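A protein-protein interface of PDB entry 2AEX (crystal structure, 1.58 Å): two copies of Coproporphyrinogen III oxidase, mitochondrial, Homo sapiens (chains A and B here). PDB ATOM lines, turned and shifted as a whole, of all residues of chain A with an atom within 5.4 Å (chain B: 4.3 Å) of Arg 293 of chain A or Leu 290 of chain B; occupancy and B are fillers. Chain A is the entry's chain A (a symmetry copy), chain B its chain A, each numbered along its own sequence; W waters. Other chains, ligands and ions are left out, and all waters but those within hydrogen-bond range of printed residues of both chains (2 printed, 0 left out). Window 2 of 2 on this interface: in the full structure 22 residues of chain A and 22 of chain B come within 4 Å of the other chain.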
ATOM      1  N   ASN A 288     -10.739 -22.139 -19.134  1.00  0.00           N
ATOM      2  CA  ASN A 288     -10.775 -22.615 -17.785  1.00  0.00           C
ATOM      3  C   ASN A 288     -12.206 -22.919 -17.398  1.00  0.00           C
ATOM      4  O   ASN A 288     -12.483 -23.982 -16.888  1.00  0.00           O
ATOM      5  CB  ASN A 288     -10.143 -21.583 -16.838  1.00  0.00           C
ATOM      6  CG  ASN A 288      -8.620 -21.601 -16.931  1.00  0.00           C
ATOM      7  OD1 ASN A 288      -8.007 -22.595 -16.566  1.00  0.00           O
ATOM      8  ND2 ASN A 288      -8.018 -20.541 -17.493  1.00  0.00           N
ATOM      9  N   LEU A 289     -13.094 -21.962 -17.665  1.00  0.00           N
ATOM     10  CA  LEU A 289     -14.511 -22.065 -17.264  1.00  0.00           C
ATOM     11  C   LEU A 289     -15.162 -23.377 -17.689  1.00  0.00           C
ATOM     12  O   LEU A 289     -15.921 -23.999 -16.929  1.00  0.00           O
ATOM     13  CB  LEU A 289     -15.309 -20.910 -17.872  1.00  0.00           C
ATOM     14  CG  LEU A 289     -15.300 -19.579 -17.143  1.00  0.00           C
ATOM     15  CD1 LEU A 289     -15.894 -18.480 -17.982  1.00  0.00           C
ATOM     16  CD2 LEU A 289     -16.114 -19.734 -15.862  1.00  0.00           C
ATOM     17  N   TYR A 291     -13.315 -26.074 -19.580  1.00  0.00           N
ATOM     18  CA  TYR A 291     -12.451 -27.250 -19.812  1.00  0.00           C
ATOM     19  C   TYR A 291     -11.306 -27.476 -18.831  1.00  0.00           C
ATOM     20  O   TYR A 291     -10.649 -28.519 -18.884  1.00  0.00           O
ATOM     21  CB  TYR A 291     -11.909 -27.191 -21.246  1.00  0.00           C
ATOM     22  CG  TYR A 291     -13.008 -27.096 -22.293  1.00  0.00           C
ATOM     23  CD1 TYR A 291     -13.183 -25.949 -23.058  1.00  0.00           C
ATOM     24  CD2 TYR A 291     -13.890 -28.159 -22.501  1.00  0.00           C
ATOM     25  CE1 TYR A 291     -14.224 -25.859 -24.014  1.00  0.00           C
ATOM     26  CE2 TYR A 291     -14.928 -28.080 -23.464  1.00  0.00           C
ATOM     27  CZ  TYR A 291     -15.080 -26.936 -24.217  1.00  0.00           C
ATOM     28  OH  TYR A 291     -16.089 -26.834 -25.177  1.00  0.00           O
ATOM     29  N   ASP A 292     -11.079 -26.525 -17.936  1.00  0.00           N
ATOM     30  CA  ASP A 292      -9.942 -26.581 -17.020  1.00  0.00           C
ATOM     31  C   ASP A 292     -10.274 -25.759 -15.768  1.00  0.00           C
ATOM     32  O   ASP A 292      -9.696 -24.689 -15.529  1.00  0.00           O
ATOM     33  CB  ASP A 292      -8.671 -26.073 -17.743  1.00  0.00           C
ATOM     34  CG  ASP A 292      -7.412 -26.156 -16.878  1.00  0.00           C
ATOM     35  OD1 ASP A 292      -7.385 -26.961 -15.932  1.00  0.00           O
ATOM     36  OD2 ASP A 292      -6.453 -25.389 -17.134  1.00  0.00           O
ATOM     37  N   ARG A 293     -11.213 -26.279 -14.973  1.00  0.00           N
ATOM     38  CA  ARG A 293     -11.826 -25.521 -13.872  1.00  0.00           C
ATOM     39  C   ARG A 293     -11.100 -25.571 -12.572  1.00  0.00           C
ATOM     40  O   ARG A 293     -11.458 -24.844 -11.645  1.00  0.00           O
ATOM     41  CB  ARG A 293     -13.197 -26.069 -13.531  1.00  0.00           C
ATOM     42  CG  ARG A 293     -13.206 -27.386 -12.688  1.00  0.00           C
ATOM     43  CD  ARG A 293     -14.284 -27.460 -11.556  1.00  0.00           C
ATOM     44  NE  ARG A 293     -13.729 -27.246 -10.212  1.00  0.00           N
ATOM     45  CZ  ARG A 293     -14.274 -27.676  -9.069  1.00  0.00           C
ATOM     46  NH1 ARG A 293     -15.412 -28.372  -9.058  1.00  0.00           N
ATOM     47  NH2 ARG A 293     -13.667 -27.417  -7.911  1.00  0.00           N
ATOM     48  N   GLY A 294     -10.155 -26.487 -12.454  1.00  0.00           N
ATOM     49  CA  GLY A 294      -9.451 -26.638 -11.204  1.00  0.00           C
ATOM     50  C   GLY A 294      -9.309 -28.090 -10.862  1.00  0.00           C
ATOM     51  O   GLY A 294     -10.286 -28.846 -10.868  1.00  0.00           O
ATOM     52  N   THR A 295      -8.070 -28.490 -10.612  1.00  0.00           N
ATOM     53  CA  THR A 295      -7.795 -29.779  -9.987  1.00  0.00           C
ATOM     54  C   THR A 295      -6.749 -29.579  -8.909  1.00  0.00           C
ATOM     55  O   THR A 295      -5.746 -28.890  -9.129  1.00  0.00           O
ATOM     56  CB  THR A 295      -7.329 -30.854 -10.982  1.00  0.00           C
ATOM     57  OG1 THR A 295      -6.837 -31.989 -10.247  1.00  0.00           O
ATOM     58  CG2 THR A 295      -6.242 -30.329 -11.927  1.00  0.00           C
ATOM     59  N   SER A 304      -5.114 -27.280 -14.199  1.00  0.00           N
ATOM     60  CA  SER A 304      -4.637 -26.209 -13.339  1.00  0.00           C
ATOM     61  C   SER A 304      -5.212 -26.296 -11.925  1.00  0.00           C
ATOM     62  O   SER A 304      -6.392 -26.590 -11.759  1.00  0.00           O
ATOM     63  CB  SER A 304      -5.106 -24.877 -13.928  1.00  0.00           C
ATOM     64  OG  SER A 304      -4.599 -24.660 -15.230  1.00  0.00           O
ATOM     65  N   ILE A 306      -6.564 -24.187  -8.594  1.00  0.00           N
ATOM     66  CA  ILE A 306      -7.324 -22.931  -8.415  1.00  0.00           C
ATOM     67  C   ILE A 306      -6.395 -21.698  -8.373  1.00  0.00           C
ATOM     68  O   ILE A 306      -6.631 -20.671  -9.024  1.00  0.00           O
ATOM     69  CB  ILE A 306      -8.302 -23.016  -7.166  1.00  0.00           C
ATOM     70  CG1 ILE A 306      -8.744 -21.637  -6.660  1.00  0.00           C
ATOM     71  CG2 ILE A 306      -7.671 -23.722  -5.976  1.00  0.00           C
ATOM     72  CD1 ILE A 306     -10.014 -21.705  -5.762  1.00  0.00           C
ATOM     73  N   ILE A 309      -5.341 -20.850 -11.872  1.00  0.00           N
ATOM     74  CA  ILE A 309      -6.458 -20.287 -12.622  1.00  0.00           C
ATOM     75  C   ILE A 309      -6.647 -18.828 -12.232  1.00  0.00           C
ATOM     76  O   ILE A 309      -6.802 -17.975 -13.095  1.00  0.00           O
ATOM     77  CB  ILE A 309      -7.748 -21.039 -12.385  1.00  0.00           C
ATOM     78  CG1 ILE A 309      -7.643 -22.455 -12.943  1.00  0.00           C
ATOM     79  CG2 ILE A 309      -8.950 -20.296 -13.032  1.00  0.00           C
ATOM     80  CD1 ILE A 309      -8.853 -23.273 -12.635  1.00  0.00           C
ATOM     81  N   LEU A 310      -6.601 -18.532 -10.945  1.00  0.00           N
ATOM     82  CA  LEU A 310      -6.767 -17.146 -10.525  1.00  0.00           C
ATOM     83  C   LEU A 310      -5.660 -16.258 -11.066  1.00  0.00           C
ATOM     84  O   LEU A 310      -5.907 -15.144 -11.536  1.00  0.00           O
ATOM     85  CB  LEU A 310      -6.863 -17.031  -9.001  1.00  0.00           C
ATOM     86  CG  LEU A 310      -8.039 -17.744  -8.346  1.00  0.00           C
ATOM     87  CD1 LEU A 310      -8.005 -17.569  -6.844  1.00  0.00           C
ATOM     88  CD2 LEU A 310      -9.330 -17.243  -8.890  1.00  0.00           C
ATOM     89  N   HIS B 219     -12.590 -20.020  -1.387  1.00  0.00           N
ATOM     90  CA  HIS B 219     -11.257 -19.500  -1.085  1.00  0.00           C
ATOM     91  C   HIS B 219     -11.240 -18.043  -0.576  1.00  0.00           C
ATOM     92  O   HIS B 219     -10.291 -17.634   0.120  1.00  0.00           O
ATOM     93  CB  HIS B 219     -10.357 -19.671  -2.303  1.00  0.00           C
ATOM     94  CG  HIS B 219     -10.476 -18.573  -3.306  1.00  0.00           C
ATOM     95  ND1 HIS B 219     -11.335 -18.636  -4.381  1.00  0.00           N
ATOM     96  CD2 HIS B 219      -9.805 -17.404  -3.423  1.00  0.00           C
ATOM     97  CE1 HIS B 219     -11.208 -17.536  -5.103  1.00  0.00           C
ATOM     98  NE2 HIS B 219     -10.285 -16.773  -4.546  1.00  0.00           N
ATOM     99  N   GLU B 286     -16.123 -16.148 -11.545  1.00  0.00           N
ATOM    100  CA  GLU B 286     -15.198 -16.978 -10.768  1.00  0.00           C
ATOM    101  C   GLU B 286     -15.893 -18.119 -10.051  1.00  0.00           C
ATOM    102  O   GLU B 286     -15.313 -19.186  -9.840  1.00  0.00           O
ATOM    103  CB  GLU B 286     -14.470 -16.084  -9.772  1.00  0.00           C
ATOM    104  CG  GLU B 286     -13.213 -16.603  -9.212  1.00  0.00           C
ATOM    105  CD  GLU B 286     -12.577 -15.614  -8.305  1.00  0.00           C
ATOM    106  OE1 GLU B 286     -12.558 -15.877  -7.102  1.00  0.00           O
ATOM    107  OE2 GLU B 286     -12.127 -14.542  -8.792  1.00  0.00           O
ATOM    108  N   PHE B 287     -17.158 -17.943  -9.666  1.00  0.00           N
ATOM    109  CA  PHE B 287     -17.876 -19.055  -9.052  1.00  0.00           C
ATOM    110  C   PHE B 287     -17.923 -20.255  -9.977  1.00  0.00           C
ATOM    111  O   PHE B 287     -17.735 -21.376  -9.529  1.00  0.00           O
ATOM    112  CB  PHE B 287     -19.282 -18.651  -8.570  1.00  0.00           C
ATOM    113  CG  PHE B 287     -20.049 -19.788  -7.981  1.00  0.00           C
ATOM    114  CD1 PHE B 287     -19.734 -20.261  -6.712  1.00  0.00           C
ATOM    115  CD2 PHE B 287     -21.038 -20.427  -8.702  1.00  0.00           C
ATOM    116  CE1 PHE B 287     -20.406 -21.358  -6.180  1.00  0.00           C
ATOM    117  CE2 PHE B 287     -21.718 -21.513  -8.173  1.00  0.00           C
ATOM    118  CZ  PHE B 287     -21.399 -21.964  -6.894  1.00  0.00           C
ATOM    119  N   ASN B 288     -18.094 -20.030 -11.281  1.00  0.00           N
ATOM    120  CA  ASN B 288     -18.088 -21.086 -12.246  1.00  0.00           C
ATOM    121  C   ASN B 288     -16.673 -21.589 -12.432  1.00  0.00           C
ATOM    122  O   ASN B 288     -16.441 -22.777 -12.379  1.00  0.00           O
ATOM    123  CB  ASN B 288     -18.691 -20.598 -13.574  1.00  0.00           C
ATOM    124  CG  ASN B 288     -20.212 -20.514 -13.497  1.00  0.00           C
ATOM    125  OD1 ASN B 288     -20.865 -21.540 -13.357  1.00  0.00           O
ATOM    126  ND2 ASN B 288     -20.770 -19.293 -13.506  1.00  0.00           N
ATOM    127  N   LEU B 289     -15.748 -20.653 -12.638  1.00  0.00           N
ATOM    128  CA  LEU B 289     -14.340 -20.985 -12.930  1.00  0.00           C
ATOM    129  C   LEU B 289     -13.734 -21.965 -11.932  1.00  0.00           C
ATOM    130  O   LEU B 289     -13.005 -22.899 -12.303  1.00  0.00           O
ATOM    131  CB  LEU B 289     -13.494 -19.710 -12.931  1.00  0.00           C
ATOM    132  CG  LEU B 289     -13.461 -18.879 -14.200  1.00  0.00           C
ATOM    133  CD1 LEU B 289     -12.819 -17.537 -13.971  1.00  0.00           C
ATOM    134  CD2 LEU B 289     -12.665 -19.648 -15.250  1.00  0.00           C
ATOM    135  N   LEU B 290     -14.023 -21.727 -10.666  1.00  0.00           N
ATOM    136  CA  LEU B 290     -13.461 -22.510  -9.586  1.00  0.00           C
ATOM    137  C   LEU B 290     -14.371 -23.663  -9.188  1.00  0.00           C
ATOM    138  O   LEU B 290     -13.913 -24.792  -9.098  1.00  0.00           O
ATOM    139  CB  LEU B 290     -13.204 -21.612  -8.381  1.00  0.00           C
ATOM    140  CG  LEU B 290     -12.396 -20.340  -8.659  1.00  0.00           C
ATOM    141  CD1 LEU B 290     -12.299 -19.510  -7.385  1.00  0.00           C
ATOM    142  CD2 LEU B 290     -11.011 -20.647  -9.246  1.00  0.00           C
ATOM    143  N   TYR B 291     -15.662 -23.385  -9.012  1.00  0.00           N
ATOM    144  CA  TYR B 291     -16.566 -24.279  -8.261  1.00  0.00           C
ATOM    145  C   TYR B 291     -17.728 -24.899  -9.031  1.00  0.00           C
ATOM    146  O   TYR B 291     -18.423 -25.769  -8.499  1.00  0.00           O
ATOM    147  CB  TYR B 291     -17.093 -23.533  -7.029  1.00  0.00           C
ATOM    148  CG  TYR B 291     -15.981 -22.997  -6.140  1.00  0.00           C
ATOM    149  CD1 TYR B 291     -15.757 -21.632  -6.003  1.00  0.00           C
ATOM    150  CD2 TYR B 291     -15.137 -23.869  -5.447  1.00  0.00           C
ATOM    151  CE1 TYR B 291     -14.704 -21.142  -5.192  1.00  0.00           C
ATOM    152  CE2 TYR B 291     -14.088 -23.385  -4.626  1.00  0.00           C
ATOM    153  CZ  TYR B 291     -13.887 -22.027  -4.498  1.00  0.00           C
ATOM    154  OH  TYR B 291     -12.866 -21.523  -3.690  1.00  0.00           O
ATOM    155  N   ASP B 292     -17.927 -24.473 -10.271  1.00  0.00           N
ATOM    156  CA  ASP B 292     -19.075 -24.911 -11.063  1.00  0.00           C
ATOM    157  C   ASP B 292     -18.724 -24.788 -12.551  1.00  0.00           C
ATOM    158  O   ASP B 292     -19.265 -23.936 -13.270  1.00  0.00           O
ATOM    159  CB  ASP B 292     -20.319 -24.076 -10.675  1.00  0.00           C
ATOM    160  CG  ASP B 292     -21.588 -24.510 -11.411  1.00  0.00           C
ATOM    161  OD1 ASP B 292     -21.654 -25.664 -11.867  1.00  0.00           O
ATOM    162  OD2 ASP B 292     -22.516 -23.678 -11.555  1.00  0.00           O
ATOM    163  N   ARG B 293     -17.813 -25.656 -12.999  1.00  0.00           N
ATOM    164  CA  ARG B 293     -17.182 -25.529 -14.321  1.00  0.00           C
ATOM    165  C   ARG B 293     -17.921 -26.158 -15.452  1.00  0.00           C
ATOM    166  O   ARG B 293     -17.545 -25.966 -16.609  1.00  0.00           O
ATOM    167  CB  ARG B 293     -15.835 -26.223 -14.352  1.00  0.00           C
ATOM    168  CG  ARG B 293     -15.883 -27.780 -14.476  1.00  0.00           C
ATOM    169  CD  ARG B 293     -14.819 -28.418 -15.430  1.00  0.00           C
ATOM    170  NE  ARG B 293     -15.378 -28.842 -16.721  1.00  0.00           N
ATOM    171  CZ  ARG B 293     -14.860 -29.779 -17.522  1.00  0.00           C
ATOM    172  NH1 ARG B 293     -13.749 -30.440 -17.194  1.00  0.00           N
ATOM    173  NH2 ARG B 293     -15.468 -30.073 -18.672  1.00  0.00           N
HETATM  174  O   HOH W   1     -11.833 -29.076 -15.086  1.00  0.00           O
HETATM  175  O   HOH W   2     -17.295 -28.091 -11.577  1.00  0.00           O
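The backbone carbonyl oxygen (O) of Leu 289 of chain B sits close to the backbone carbonyl oxygen (O) of Arg 293 of chain A. O of Leu 290 of chain B is in hydrogen-bond range of NE of Arg 293 of chain A (2.7 Å). O of Arg 293 of chain B lies close to O of Leu 289 of chain A, 2.6 Å away.
Of the 9 printed residues of chain B, 7 touch a printed residue of chain A. Printed residues of chain B that touch a printed residue of chain A: His 219, Glu 286, Asn 288, Leu 289, Leu 290, Tyr 291 and Arg 293. Among the printed residues, 13 pairs touch across the chains.
The side-chain amide oxygen (OD1) of Asn 288 of chain B sits close to the backbone carbonyl oxygen (O) of Asp 292 of chain B. OH of Tyr 291 of chain B lies within hydrogen-bond range of N of His 219 of chain B, 2.8 Å away. The backbone carbonyl oxygen (O) of Asn 288 of chain A lies within hydrogen-bond range of the backbone NH (N) of Arg 293 of chain A (3.2 Å). The side-chain amide oxygen (OD1) of Asn 288 of chain A sits close to the backbone carbonyl oxygen (O) of Asp 292 of chain A (2.9 Å). O of Asn 288 of chain B is in hydrogen-bond range of N of Arg 293 of chain B (3.2 Å).
Among the printed residues, merely in contact across the chains: Arg 293 of chain A with Arg 293 of chain B (2.8 Å), Leu 289 of chain A with Leu 289 of chain B (3.2 Å), Leu 310 of chain A with His 219 of chain B (3.3 Å), Ile 306 of chain A with Tyr 291 of chain B (3.5 Å), Leu 289 of chain A with Asn 288 of chain B (3.6 Å), Asn 288 of chain A with Leu 289 of chain B (3.6 Å), Ile 306 of chain A with Leu 290 of chain B (3.6 Å), Ile 306 of chain A with His 219 of chain B (3.6 Å), Leu 310 of chain A with Glu 286 of chain B (3.7 Å) and Leu 310 of chain A with Leu 290 of chain B (3.8 Å).
Asn 288 of chain A touches Leu 289 of chain B, and with the chains exchanged Leu 289 of chain A touches Asn 288 of chain B. Leu 289 of chain B touches its own counterpart, Leu 289 of chain A. Leu 289 of chain A touches Arg 293 of chain B, and with the chains exchanged Arg 293 of chain A touches Leu 289 of chain B. Arg 293 of chain A touches its own counterpart, Arg 293 of chain B. Positions printed for both chains: 288, 289, 291, 292 and 293. Of the 13 pairs that touch across the chains among the printed residues, 6 have their exchanged pair printed and touching as well.
Printed residues of chain B within 4 Å of Arg 293 of chain A: Leu 289 (2.6 Å), Leu 290 (2.7 Å) and Arg 293 (2.8 Å). Of the printed residues of chain A, Leu 290 of chain B touches Arg 293, Ile 306 and Leu 310. Of the printed residues of chain B, Asn 288 of chain A touches Leu 289 (3.6 Å). Printed residues of chain A within 4 Å of His 219 of chain B: Ile 306 (3.6 Å) and Leu 310 (3.3 Å). Printed residues of chain A within 4 Å of Glu 286 of chain B: Leu 310. Of the printed residues of chain B, Leu 289 of chain A touches Asn 288, Leu 289 and Arg 293.
Water W2 lies within hydrogen-bond range of the backbone NH (N) of Arg 293 of chain B (2.9 Å) and the guanidinium group (NH1) of Arg 293 of chain A (3.2 Å). Water W1 lies within hydrogen-bond range of N of Arg 293 of chain A (2.9 Å) and NH1 of Arg 293 of chain B (3.2 Å).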
